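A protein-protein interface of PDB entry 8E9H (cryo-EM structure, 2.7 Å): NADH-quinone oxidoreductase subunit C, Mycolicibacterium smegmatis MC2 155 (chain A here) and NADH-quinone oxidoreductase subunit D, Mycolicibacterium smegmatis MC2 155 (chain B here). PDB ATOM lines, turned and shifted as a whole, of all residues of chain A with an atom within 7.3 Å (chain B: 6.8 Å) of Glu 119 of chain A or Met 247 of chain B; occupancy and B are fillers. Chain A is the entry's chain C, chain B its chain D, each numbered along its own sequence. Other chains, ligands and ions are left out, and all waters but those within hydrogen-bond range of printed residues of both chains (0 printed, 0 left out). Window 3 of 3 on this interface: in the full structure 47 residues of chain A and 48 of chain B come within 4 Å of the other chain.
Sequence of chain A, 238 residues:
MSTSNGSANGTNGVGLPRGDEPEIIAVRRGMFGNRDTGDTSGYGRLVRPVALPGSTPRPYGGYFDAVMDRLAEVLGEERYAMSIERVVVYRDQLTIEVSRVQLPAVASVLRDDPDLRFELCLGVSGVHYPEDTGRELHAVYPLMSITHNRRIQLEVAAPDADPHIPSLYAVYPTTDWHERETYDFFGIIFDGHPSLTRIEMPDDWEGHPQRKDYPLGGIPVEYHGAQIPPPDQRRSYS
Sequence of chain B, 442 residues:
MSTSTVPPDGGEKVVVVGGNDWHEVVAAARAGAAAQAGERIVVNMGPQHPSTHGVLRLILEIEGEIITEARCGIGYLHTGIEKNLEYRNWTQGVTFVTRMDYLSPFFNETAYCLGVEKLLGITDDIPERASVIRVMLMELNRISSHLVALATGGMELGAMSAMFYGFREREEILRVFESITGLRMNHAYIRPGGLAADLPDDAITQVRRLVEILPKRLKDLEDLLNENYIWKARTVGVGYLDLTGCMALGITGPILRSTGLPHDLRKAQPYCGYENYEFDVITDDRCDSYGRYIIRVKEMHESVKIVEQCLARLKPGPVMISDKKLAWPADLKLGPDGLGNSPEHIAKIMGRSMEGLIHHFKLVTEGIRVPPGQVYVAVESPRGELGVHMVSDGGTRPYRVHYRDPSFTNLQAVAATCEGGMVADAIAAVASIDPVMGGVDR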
ATOM      1  N   LEU A 110      15.091  -3.617   9.487  1.00  0.00           N
ATOM      2  CA  LEU A 110      14.001  -2.650   9.483  1.00  0.00           C
ATOM      3  C   LEU A 110      13.979  -1.837  10.768  1.00  0.00           C
ATOM      4  O   LEU A 110      13.749  -0.624  10.737  1.00  0.00           O
ATOM      5  CB  LEU A 110      12.669  -3.370   9.288  1.00  0.00           C
ATOM      6  CG  LEU A 110      12.422  -3.898   7.877  1.00  0.00           C
ATOM      7  CD1 LEU A 110      11.463  -5.063   7.913  1.00  0.00           C
ATOM      8  CD2 LEU A 110      11.885  -2.793   6.994  1.00  0.00           C
ATOM      9  N   ARG A 111      14.210  -2.487  11.907  1.00  0.00           N
ATOM     10  CA  ARG A 111      14.136  -1.776  13.178  1.00  0.00           C
ATOM     11  C   ARG A 111      15.304  -0.813  13.343  1.00  0.00           C
ATOM     12  O   ARG A 111      15.115   0.347  13.726  1.00  0.00           O
ATOM     13  CB  ARG A 111      14.107  -2.775  14.331  1.00  0.00           C
ATOM     14  CG  ARG A 111      13.760  -2.148  15.663  1.00  0.00           C
ATOM     15  CD  ARG A 111      14.107  -3.068  16.809  1.00  0.00           C
ATOM     16  NE  ARG A 111      15.548  -3.177  16.990  1.00  0.00           N
ATOM     17  CZ  ARG A 111      16.133  -3.620  18.092  1.00  0.00           C
ATOM     18  NH1 ARG A 111      15.429  -3.999  19.145  1.00  0.00           N
ATOM     19  NH2 ARG A 111      17.460  -3.684  18.140  1.00  0.00           N
ATOM     20  N   ASP A 112      16.518  -1.273  13.055  1.00  0.00           N
ATOM     21  CA  ASP A 112      17.719  -0.540  13.428  1.00  0.00           C
ATOM     22  C   ASP A 112      18.136   0.495  12.392  1.00  0.00           C
ATOM     23  O   ASP A 112      18.659   1.551  12.759  1.00  0.00           O
ATOM     24  CB  ASP A 112      18.866  -1.521  13.664  1.00  0.00           C
ATOM     25  CG  ASP A 112      18.573  -2.497  14.784  1.00  0.00           C
ATOM     26  OD1 ASP A 112      17.650  -2.231  15.580  1.00  0.00           O
ATOM     27  OD2 ASP A 112      19.266  -3.532  14.867  1.00  0.00           O
ATOM     28  N   ASP A 113      17.924   0.222  11.113  1.00  0.00           N
ATOM     29  CA  ASP A 113      18.426   1.119  10.084  1.00  0.00           C
ATOM     30  C   ASP A 113      17.799   2.502  10.244  1.00  0.00           C
ATOM     31  O   ASP A 113      16.572   2.607  10.365  1.00  0.00           O
ATOM     32  CB  ASP A 113      18.122   0.570   8.696  1.00  0.00           C
ATOM     33  CG  ASP A 113      18.626   1.475   7.599  1.00  0.00           C
ATOM     34  OD1 ASP A 113      19.855   1.529   7.391  1.00  0.00           O
ATOM     35  OD2 ASP A 113      17.796   2.142   6.950  1.00  0.00           O
ATOM     36  N   LEU A 116      14.975   3.195   7.687  1.00  0.00           N
ATOM     37  CA  LEU A 116      13.782   2.373   7.861  1.00  0.00           C
ATOM     38  C   LEU A 116      13.172   2.593   9.241  1.00  0.00           C
ATOM     39  O   LEU A 116      12.045   3.081   9.358  1.00  0.00           O
ATOM     40  CB  LEU A 116      14.132   0.897   7.660  1.00  0.00           C
ATOM     41  CG  LEU A 116      14.711   0.535   6.297  1.00  0.00           C
ATOM     42  CD1 LEU A 116      15.282  -0.868   6.320  1.00  0.00           C
ATOM     43  CD2 LEU A 116      13.650   0.662   5.230  1.00  0.00           C
ATOM     44  N   ARG A 117      13.918   2.252  10.289  1.00  0.00           N
ATOM     45  CA  ARG A 117      13.546   2.600  11.653  1.00  0.00           C
ATOM     46  C   ARG A 117      12.088   2.277  11.951  1.00  0.00           C
ATOM     47  O   ARG A 117      11.292   3.180  12.222  1.00  0.00           O
ATOM     48  CB  ARG A 117      13.824   4.087  11.890  1.00  0.00           C
ATOM     49  CG  ARG A 117      13.609   4.582  13.313  1.00  0.00           C
ATOM     50  CD  ARG A 117      14.093   3.603  14.367  1.00  0.00           C
ATOM     51  NE  ARG A 117      15.503   3.274  14.204  1.00  0.00           N
ATOM     52  CZ  ARG A 117      16.502   4.076  14.539  1.00  0.00           C
ATOM     53  NH1 ARG A 117      16.284   5.279  15.045  1.00  0.00           N
ATOM     54  NH2 ARG A 117      17.754   3.662  14.363  1.00  0.00           N
ATOM     55  N   PHE A 118      11.725   0.998  11.892  1.00  0.00           N
ATOM     56  CA  PHE A 118      10.379   0.560  12.264  1.00  0.00           C
ATOM     57  C   PHE A 118      10.399   0.087  13.716  1.00  0.00           C
ATOM     58  O   PHE A 118      10.328  -1.101  14.030  1.00  0.00           O
ATOM     59  CB  PHE A 118       9.893  -0.531  11.322  1.00  0.00           C
ATOM     60  CG  PHE A 118       9.588  -0.041   9.942  1.00  0.00           C
ATOM     61  CD1 PHE A 118       8.354   0.498   9.643  1.00  0.00           C
ATOM     62  CD2 PHE A 118      10.536  -0.118   8.944  1.00  0.00           C
ATOM     63  CE1 PHE A 118       8.075   0.952   8.376  1.00  0.00           C
ATOM     64  CE2 PHE A 118      10.260   0.332   7.676  1.00  0.00           C
ATOM     65  CZ  PHE A 118       9.028   0.868   7.391  1.00  0.00           C
ATOM     66  N   GLU A 119      10.496   1.064  14.616  1.00  0.00           N
ATOM     67  CA  GLU A 119      10.692   0.750  16.025  1.00  0.00           C
ATOM     68  C   GLU A 119       9.499   0.017  16.618  1.00  0.00           C
ATOM     69  O   GLU A 119       9.662  -0.775  17.553  1.00  0.00           O
ATOM     70  CB  GLU A 119      10.961   2.029  16.818  1.00  0.00           C
ATOM     71  CG  GLU A 119       9.851   3.068  16.736  1.00  0.00           C
ATOM     72  CD  GLU A 119      10.006   4.008  15.563  1.00  0.00           C
ATOM     73  OE1 GLU A 119      11.073   3.985  14.922  1.00  0.00           O
ATOM     74  OE2 GLU A 119       9.058   4.768  15.275  1.00  0.00           O
ATOM     75  N   LEU A 120       8.301   0.261  16.103  1.00  0.00           N
ATOM     76  CA  LEU A 120       7.066  -0.223  16.714  1.00  0.00           C
ATOM     77  C   LEU A 120       6.522  -1.392  15.899  1.00  0.00           C
ATOM     78  O   LEU A 120       5.912  -1.202  14.847  1.00  0.00           O
ATOM     79  CB  LEU A 120       6.046   0.900  16.810  1.00  0.00           C
ATOM     80  CG  LEU A 120       4.789   0.581  17.614  1.00  0.00           C
ATOM     81  CD1 LEU A 120       5.002   0.923  19.070  1.00  0.00           C
ATOM     82  CD2 LEU A 120       3.601   1.339  17.062  1.00  0.00           C
ATOM     83  N   CYS A 121       6.752  -2.605  16.391  1.00  0.00           N
ATOM     84  CA  CYS A 121       6.033  -3.763  15.881  1.00  0.00           C
ATOM     85  C   CYS A 121       4.725  -3.905  16.638  1.00  0.00           C
ATOM     86  O   CYS A 121       4.714  -3.961  17.870  1.00  0.00           O
ATOM     87  CB  CYS A 121       6.865  -5.030  16.033  1.00  0.00           C
ATOM     88  SG  CYS A 121       5.981  -6.535  15.582  1.00  0.00           S
ATOM     89  N   LEU A 122       3.619  -3.961  15.906  1.00  0.00           N
ATOM     90  CA  LEU A 122       2.313  -3.896  16.540  1.00  0.00           C
ATOM     91  C   LEU A 122       1.788  -5.250  16.983  1.00  0.00           C
ATOM     92  O   LEU A 122       0.823  -5.299  17.751  1.00  0.00           O
ATOM     93  CB  LEU A 122       1.311  -3.240  15.592  1.00  0.00           C
ATOM     94  CG  LEU A 122       1.530  -1.736  15.471  1.00  0.00           C
ATOM     95  CD1 LEU A 122       1.107  -1.261  14.105  1.00  0.00           C
ATOM     96  CD2 LEU A 122       0.783  -0.993  16.556  1.00  0.00           C
ATOM     97  N   LEU A 143       4.307  -3.580  11.176  1.00  0.00           N
ATOM     98  CA  LEU A 143       5.355  -2.714  11.685  1.00  0.00           C
ATOM     99  C   LEU A 143       5.032  -1.268  11.350  1.00  0.00           C
ATOM    100  O   LEU A 143       4.566  -0.964  10.245  1.00  0.00           O
ATOM    101  CB  LEU A 143       6.711  -3.085  11.095  1.00  0.00           C
ATOM    102  CG  LEU A 143       7.086  -4.557  11.208  1.00  0.00           C
ATOM    103  CD1 LEU A 143       8.450  -4.793  10.606  1.00  0.00           C
ATOM    104  CD2 LEU A 143       7.058  -4.996  12.654  1.00  0.00           C
ATOM    105  N   MET A 144       5.273  -0.385  12.311  1.00  0.00           N
ATOM    106  CA  MET A 144       5.098   1.045  12.129  1.00  0.00           C
ATOM    107  C   MET A 144       6.369   1.767  12.532  1.00  0.00           C
ATOM    108  O   MET A 144       6.981   1.447  13.553  1.00  0.00           O
ATOM    109  CB  MET A 144       3.928   1.584  12.952  1.00  0.00           C
ATOM    110  CG  MET A 144       3.503   2.976  12.532  1.00  0.00           C
ATOM    111  SD  MET A 144       2.589   3.892  13.776  1.00  0.00           S
ATOM    112  CE  MET A 144       2.153   5.347  12.830  1.00  0.00           C
ATOM    113  N   SER A 145       6.761   2.736  11.717  1.00  0.00           N
ATOM    114  CA  SER A 145       7.852   3.643  12.030  1.00  0.00           C
ATOM    115  C   SER A 145       7.256   4.993  12.394  1.00  0.00           C
ATOM    116  O   SER A 145       6.764   5.714  11.517  1.00  0.00           O
ATOM    117  CB  SER A 145       8.806   3.782  10.847  1.00  0.00           C
ATOM    118  OG  SER A 145       9.771   4.785  11.096  1.00  0.00           O
ATOM    119  N   ILE A 146       7.284   5.325  13.685  1.00  0.00           N
ATOM    120  CA  ILE A 146       6.772   6.618  14.121  1.00  0.00           C
ATOM    121  C   ILE A 146       7.668   7.741  13.627  1.00  0.00           C
ATOM    122  O   ILE A 146       7.186   8.818  13.262  1.00  0.00           O
ATOM    123  CB  ILE A 146       6.625   6.650  15.651  1.00  0.00           C
ATOM    124  CG1 ILE A 146       5.616   5.601  16.110  1.00  0.00           C
ATOM    125  CG2 ILE A 146       6.191   8.030  16.107  1.00  0.00           C
ATOM    126  CD1 ILE A 146       6.248   4.371  16.690  1.00  0.00           C
ATOM    127  N   THR A 147       8.982   7.515  13.613  1.00  0.00           N
ATOM    128  CA  THR A 147       9.904   8.555  13.171  1.00  0.00           C
ATOM    129  C   THR A 147       9.546   9.039  11.774  1.00  0.00           C
ATOM    130  O   THR A 147       9.377  10.241  11.543  1.00  0.00           O
ATOM    131  CB  THR A 147      11.338   8.030  13.200  1.00  0.00           C
ATOM    132  OG1 THR A 147      11.473   6.960  12.259  1.00  0.00           O
ATOM    133  CG2 THR A 147      11.700   7.526  14.583  1.00  0.00           C
ATOM    134  N   HIS A 148       9.416   8.111  10.829  1.00  0.00           N
ATOM    135  CA  HIS A 148       9.064   8.447   9.460  1.00  0.00           C
ATOM    136  C   HIS A 148       7.570   8.380   9.197  1.00  0.00           C
ATOM    137  O   HIS A 148       7.135   8.734   8.098  1.00  0.00           O
ATOM    138  CB  HIS A 148       9.784   7.507   8.489  1.00  0.00           C
ATOM    139  CG  HIS A 148      11.267   7.476   8.676  1.00  0.00           C
ATOM    140  ND1 HIS A 148      12.055   8.597   8.544  1.00  0.00           N
ATOM    141  CD2 HIS A 148      12.103   6.461   8.990  1.00  0.00           C
ATOM    142  CE1 HIS A 148      13.316   8.273   8.767  1.00  0.00           C
ATOM    143  NE2 HIS A 148      13.372   6.982   9.039  1.00  0.00           N
ATOM    144  N   ASN A 149       6.777   7.941  10.168  1.00  0.00           N
ATOM    145  CA  ASN A 149       5.338   7.804   9.997  1.00  0.00           C
ATOM    146  C   ASN A 149       5.030   6.924   8.788  1.00  0.00           C
ATOM    147  O   ASN A 149       4.403   7.341   7.817  1.00  0.00           O
ATOM    148  CB  ASN A 149       4.677   9.175   9.860  1.00  0.00           C
ATOM    149  CG  ASN A 149       3.180   9.081   9.730  1.00  0.00           C
ATOM    150  OD1 ASN A 149       2.582   8.065  10.074  1.00  0.00           O
ATOM    151  ND2 ASN A 149       2.561  10.141   9.233  1.00  0.00           N
ATOM    152  N   ARG A 150       5.495   5.682   8.869  1.00  0.00           N
ATOM    153  CA  ARG A 150       5.329   4.717   7.794  1.00  0.00           C
ATOM    154  C   ARG A 150       4.779   3.421   8.362  1.00  0.00           C
ATOM    155  O   ARG A 150       4.943   3.131   9.546  1.00  0.00           O
ATOM    156  CB  ARG A 150       6.649   4.445   7.082  1.00  0.00           C
ATOM    157  CG  ARG A 150       7.187   5.637   6.328  1.00  0.00           C
ATOM    158  CD  ARG A 150       8.511   5.319   5.676  1.00  0.00           C
ATOM    159  NE  ARG A 150       9.031   6.461   4.941  1.00  0.00           N
ATOM    160  CZ  ARG A 150      10.230   6.505   4.380  1.00  0.00           C
ATOM    161  NH1 ARG A 150      11.067   5.485   4.455  1.00  0.00           N
ATOM    162  NH2 ARG A 150      10.599   7.603   3.726  1.00  0.00           N
ATOM    163  N   VAL A 171      14.412  -8.938  18.536  1.00  0.00           N
ATOM    164  CA  VAL A 171      14.259  -7.673  17.827  1.00  0.00           C
ATOM    165  C   VAL A 171      13.068  -6.889  18.351  1.00  0.00           C
ATOM    166  O   VAL A 171      13.183  -5.703  18.669  1.00  0.00           O
ATOM    167  CB  VAL A 171      14.128  -7.935  16.315  1.00  0.00           C
ATOM    168  CG1 VAL A 171      14.144  -6.630  15.553  1.00  0.00           C
ATOM    169  CG2 VAL A 171      15.239  -8.853  15.841  1.00  0.00           C
ATOM    170  N   TYR A 172      11.908  -7.534  18.445  1.00  0.00           N
ATOM    171  CA  TYR A 172      10.673  -6.897  18.893  1.00  0.00           C
ATOM    172  C   TYR A 172      10.140  -7.664  20.092  1.00  0.00           C
ATOM    173  O   TYR A 172       9.409  -8.651  19.934  1.00  0.00           O
ATOM    174  CB  TYR A 172       9.639  -6.852  17.775  1.00  0.00           C
ATOM    175  CG  TYR A 172       9.989  -5.896  16.667  1.00  0.00           C
ATOM    176  CD1 TYR A 172      10.078  -4.536  16.904  1.00  0.00           C
ATOM    177  CD2 TYR A 172      10.236  -6.354  15.385  1.00  0.00           C
ATOM    178  CE1 TYR A 172      10.397  -3.660  15.895  1.00  0.00           C
ATOM    179  CE2 TYR A 172      10.555  -5.485  14.370  1.00  0.00           C
ATOM    180  CZ  TYR A 172      10.634  -4.139  14.631  1.00  0.00           C
ATOM    181  OH  TYR A 172      10.955  -3.266  13.622  1.00  0.00           O
ATOM    182  N   PRO A 173      10.479  -7.241  21.310  1.00  0.00           N
ATOM    183  CA  PRO A 173       9.960  -7.949  22.487  1.00  0.00           C
ATOM    184  C   PRO A 173       8.450  -8.007  22.520  1.00  0.00           C
ATOM    185  O   PRO A 173       7.884  -8.954  23.076  1.00  0.00           O
ATOM    186  CB  PRO A 173      10.516  -7.130  23.656  1.00  0.00           C
ATOM    187  CG  PRO A 173      11.708  -6.454  23.108  1.00  0.00           C
ATOM    188  CD  PRO A 173      11.375  -6.139  21.687  1.00  0.00           C
ATOM    189  N   THR A 174       7.778  -7.016  21.939  1.00  0.00           N
ATOM    190  CA  THR A 174       6.324  -7.013  21.936  1.00  0.00           C
ATOM    191  C   THR A 174       5.755  -8.259  21.283  1.00  0.00           C
ATOM    192  O   THR A 174       4.627  -8.649  21.597  1.00  0.00           O
ATOM    193  CB  THR A 174       5.806  -5.776  21.212  1.00  0.00           C
ATOM    194  OG1 THR A 174       4.398  -5.645  21.434  1.00  0.00           O
ATOM    195  CG2 THR A 174       6.070  -5.886  19.728  1.00  0.00           C
ATOM    196  N   ASP B 242       9.295   4.390  30.641  1.00  0.00           N
ATOM    197  CA  ASP B 242       9.913   5.347  29.740  1.00  0.00           C
ATOM    198  C   ASP B 242       9.499   5.078  28.298  1.00  0.00           C
ATOM    199  O   ASP B 242       8.942   4.031  27.964  1.00  0.00           O
ATOM    200  CB  ASP B 242      11.434   5.288  29.863  1.00  0.00           C
ATOM    201  N   LEU B 243       9.783   6.053  27.434  1.00  0.00           N
ATOM    202  CA  LEU B 243       9.484   5.897  26.016  1.00  0.00           C
ATOM    203  C   LEU B 243      10.135   4.642  25.455  1.00  0.00           C
ATOM    204  O   LEU B 243       9.543   3.938  24.628  1.00  0.00           O
ATOM    205  CB  LEU B 243       9.954   7.131  25.249  1.00  0.00           C
ATOM    206  CG  LEU B 243       9.432   7.294  23.824  1.00  0.00           C
ATOM    207  CD1 LEU B 243       9.383   8.762  23.458  1.00  0.00           C
ATOM    208  CD2 LEU B 243      10.299   6.544  22.842  1.00  0.00           C
ATOM    209  N   THR B 244      11.359   4.345  25.891  1.00  0.00           N
ATOM    210  CA  THR B 244      12.030   3.140  25.425  1.00  0.00           C
ATOM    211  C   THR B 244      11.216   1.903  25.761  1.00  0.00           C
ATOM    212  O   THR B 244      11.072   0.999  24.931  1.00  0.00           O
ATOM    213  CB  THR B 244      13.417   3.039  26.048  1.00  0.00           C
ATOM    214  OG1 THR B 244      14.110   4.279  25.879  1.00  0.00           O
ATOM    215  CG2 THR B 244      14.206   1.924  25.396  1.00  0.00           C
ATOM    216  N   GLY B 245      10.679   1.842  26.977  1.00  0.00           N
ATOM    217  CA  GLY B 245       9.846   0.711  27.339  1.00  0.00           C
ATOM    218  C   GLY B 245       8.595   0.624  26.492  1.00  0.00           C
ATOM    219  O   GLY B 245       8.192  -0.464  26.074  1.00  0.00           O
ATOM    220  N   CYS B 246       7.966   1.766  26.219  1.00  0.00           N
ATOM    221  CA  CYS B 246       6.767   1.757  25.392  1.00  0.00           C
ATOM    222  C   CYS B 246       7.069   1.225  23.999  1.00  0.00           C
ATOM    223  O   CYS B 246       6.307   0.417  23.458  1.00  0.00           O
ATOM    224  CB  CYS B 246       6.179   3.163  25.316  1.00  0.00           C
ATOM    225  SG  CYS B 246       5.512   3.754  26.880  1.00  0.00           S
ATOM    226  N   MET B 247       8.177   1.660  23.402  1.00  0.00           N
ATOM    227  CA  MET B 247       8.540   1.157  22.082  1.00  0.00           C
ATOM    228  C   MET B 247       8.852  -0.332  22.126  1.00  0.00           C
ATOM    229  O   MET B 247       8.378  -1.099  21.281  1.00  0.00           O
ATOM    230  CB  MET B 247       9.732   1.933  21.531  1.00  0.00           C
ATOM    231  CG  MET B 247       9.442   3.389  21.257  1.00  0.00           C
ATOM    232  SD  MET B 247       8.160   3.601  20.015  1.00  0.00           S
ATOM    233  CE  MET B 247       6.767   4.001  21.057  1.00  0.00           C
ATOM    234  N   ALA B 248       9.638  -0.765  23.111  1.00  0.00           N
ATOM    235  CA  ALA B 248      10.051  -2.162  23.151  1.00  0.00           C
ATOM    236  C   ALA B 248       8.851  -3.088  23.256  1.00  0.00           C
ATOM    237  O   ALA B 248       8.787  -4.115  22.571  1.00  0.00           O
ATOM    238  CB  ALA B 248      11.004  -2.391  24.321  1.00  0.00           C
ATOM    239  N   LEU B 249       7.887  -2.740  24.101  1.00  0.00           N
ATOM    240  CA  LEU B 249       6.688  -3.540  24.293  1.00  0.00           C
ATOM    241  C   LEU B 249       5.577  -3.165  23.328  1.00  0.00           C
ATOM    242  O   LEU B 249       4.484  -3.730  23.409  1.00  0.00           O
ATOM    243  CB  LEU B 249       6.188  -3.397  25.728  1.00  0.00           C
ATOM    244  CG  LEU B 249       7.119  -3.950  26.802  1.00  0.00           C
ATOM    245  CD1 LEU B 249       6.598  -3.613  28.182  1.00  0.00           C
ATOM    246  CD2 LEU B 249       7.284  -5.445  26.644  1.00  0.00           C
ATOM    247  N   GLY B 250       5.826  -2.230  22.417  1.00  0.00           N
ATOM    248  CA  GLY B 250       4.784  -1.805  21.507  1.00  0.00           C
ATOM    249  C   GLY B 250       3.593  -1.186  22.190  1.00  0.00           C
ATOM    250  O   GLY B 250       2.462  -1.376  21.741  1.00  0.00           O
ATOM    251  N   ILE B 251       3.813  -0.447  23.276  1.00  0.00           N
ATOM    252  CA  ILE B 251       2.713   0.207  23.968  1.00  0.00           C
ATOM    253  C   ILE B 251       2.222   1.376  23.129  1.00  0.00           C
ATOM    254  O   ILE B 251       2.965   1.939  22.315  1.00  0.00           O
ATOM    255  CB  ILE B 251       3.147   0.678  25.365  1.00  0.00           C
ATOM    256  CG1 ILE B 251       3.877  -0.431  26.123  1.00  0.00           C
ATOM    257  CG2 ILE B 251       1.945   1.126  26.158  1.00  0.00           C
ATOM    258  CD1 ILE B 251       3.023  -1.621  26.451  1.00  0.00           C
ATOM    259  N   THR B 252       0.962   1.745  23.323  1.00  0.00           N
ATOM    260  CA  THR B 252       0.350   2.835  22.581  1.00  0.00           C
ATOM    261  C   THR B 252      -0.725   3.472  23.445  1.00  0.00           C
ATOM    262  O   THR B 252      -1.004   3.026  24.559  1.00  0.00           O
ATOM    263  CB  THR B 252      -0.245   2.343  21.257  1.00  0.00           C
ATOM    264  OG1 THR B 252      -1.048   1.182  21.496  1.00  0.00           O
ATOM    265  CG2 THR B 252       0.854   2.000  20.269  1.00  0.00           C
ATOM    266  N   LEU B 256       1.710   5.421  26.052  1.00  0.00           N
ATOM    267  CA  LEU B 256       2.794   5.908  25.209  1.00  0.00           C
ATOM    268  C   LEU B 256       2.887   7.425  25.265  1.00  0.00           C
ATOM    269  O   LEU B 256       3.979   7.989  25.378  1.00  0.00           O
ATOM    270  CB  LEU B 256       2.590   5.437  23.773  1.00  0.00           C
ATOM    271  CG  LEU B 256       3.515   6.070  22.736  1.00  0.00           C
ATOM    272  CD1 LEU B 256       4.962   5.833  23.102  1.00  0.00           C
ATOM    273  CD2 LEU B 256       3.213   5.516  21.361  1.00  0.00           C
ATOM    274  N   THR B 259       4.694   9.594  27.856  1.00  0.00           N
ATOM    275  CA  THR B 259       6.136   9.737  27.747  1.00  0.00           C
ATOM    276  C   THR B 259       6.534  10.981  26.969  1.00  0.00           C
ATOM    277  O   THR B 259       7.724  11.204  26.734  1.00  0.00           O
ATOM    278  CB  THR B 259       6.737   8.499  27.089  1.00  0.00           C
ATOM    279  OG1 THR B 259       6.382   8.478  25.703  1.00  0.00           O
ATOM    280  CG2 THR B 259       6.223   7.241  27.757  1.00  0.00           C
ATOM    281  N   LEU B 261       5.743  11.567  23.814  1.00  0.00           N
ATOM    282  CA  LEU B 261       5.660  11.333  22.381  1.00  0.00           C
ATOM    283  C   LEU B 261       4.243  11.621  21.908  1.00  0.00           C
ATOM    284  O   LEU B 261       3.309  10.947  22.351  1.00  0.00           O
ATOM    285  CB  LEU B 261       6.040   9.899  22.054  1.00  0.00           C
ATOM    286  CG  LEU B 261       6.144   9.582  20.565  1.00  0.00           C
ATOM    287  CD1 LEU B 261       7.360  10.256  19.960  1.00  0.00           C
ATOM    288  CD2 LEU B 261       6.202   8.085  20.351  1.00  0.00           C
ATOM    289  N   HIS B 263       2.298  10.721  19.656  1.00  0.00           N
ATOM    290  CA  HIS B 263       1.879   9.784  18.624  1.00  0.00           C
ATOM    291  C   HIS B 263       0.391   9.505  18.753  1.00  0.00           C
ATOM    292  O   HIS B 263      -0.072   9.036  19.798  1.00  0.00           O
ATOM    293  CB  HIS B 263       2.666   8.485  18.724  1.00  0.00           C
ATOM    294  CG  HIS B 263       2.267   7.469  17.704  1.00  0.00           C
ATOM    295  ND1 HIS B 263       1.756   6.236  18.043  1.00  0.00           N
ATOM    296  CD2 HIS B 263       2.292   7.508  16.351  1.00  0.00           C
ATOM    297  CE1 HIS B 263       1.490   5.554  16.943  1.00  0.00           C
ATOM    298  NE2 HIS B 263       1.807   6.304  15.903  1.00  0.00           N
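SD of Met 144 of chain A sits close to NE2 of His 263 of chain B (3.3 Å). N of Thr 174 of chain A is in hydrogen-bond range of O of Ala 248 of chain B. The side-chain hydroxyl of Thr 174 of chain A sits at hydrogen-bond distance from the backbone carbonyl oxygen of Leu 249 of chain B (2.8 Å).
Of chain B, only Met 247 (3.7 Å) comes within 4 Å of Glu 119 of chain A. Met 247 of chain B touches just these residues of chain A: Glu 119 and Ile 146. Printed residues of chain A within 4 Å of Ala 248 of chain B: Pro 173 (3.4 Å) and Thr 174 (3.1 Å). Of the printed residues of chain B, Leu 120 of chain A touches Gly 250 (3.7 Å) and Ile 251 (3.96 Å). Printed residues of chain B within 4 Å of Ile 146 of chain A: Met 247 and His 263. Tyr 172 of chain A touches none of the printed residues of chain B.
Of the 15 printed residues of chain B, 6 touch a printed residue of chain A. Hydrophobic or aromatic side chains of chain B that line the printed part of chain A: Met 247 and His 263. Printed residues of chain A that touch a printed residue of chain B: Glu 119, Leu 120, Met 144, Ile 146, Pro 173 and Thr 174. Hydrophobic or aromatic side chains of chain A within 4 Å of the printed part of chain B: Leu 120, Met 144, Ile 146 and Pro 173. Among the printed residues, 10 pairs touch across the chains. Among the printed residues, no Asp or Glu carboxylate lies within 4 Å of a Lys or Arg side-chain nitrogen of the other chain.
The backbone NH of Ile 146 of chain A sits at hydrogen-bond distance from the side-chain carboxylate of Glu 119 of chain A (2.4 Å). The side-chain carboxylate of Glu 119 of chain A lies within hydrogen-bond range of the backbone NH of Thr 147 of chain A. The backbone carbonyl oxygen (O) of Leu 120 of chain A is in hydrogen-bond range of the backbone NH (N) of Met 144 of chain A (2.7 Å). O of Cys 246 of chain B sits at hydrogen-bond distance from N of Ile 251 of chain B (2.6 Å).
Met 247 of chain B touches Glu 119 of chain A. Leu 120 of chain A touches Gly 250 of chain B. CD1 of Leu 120 of chain A touches O of Ile 251 of chain B, at 3.96 Å. Ile 146 of chain A touches Met 247 of chain B. CD2 of His 263 of chain B touches CG1 of Ile 146 of chain A (3.8 Å). Pro 173 of chain A touches Ala 248 of chain B. Gly 250 of chain B touches Thr 174 of chain A (N to CB, 3.7 Å).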
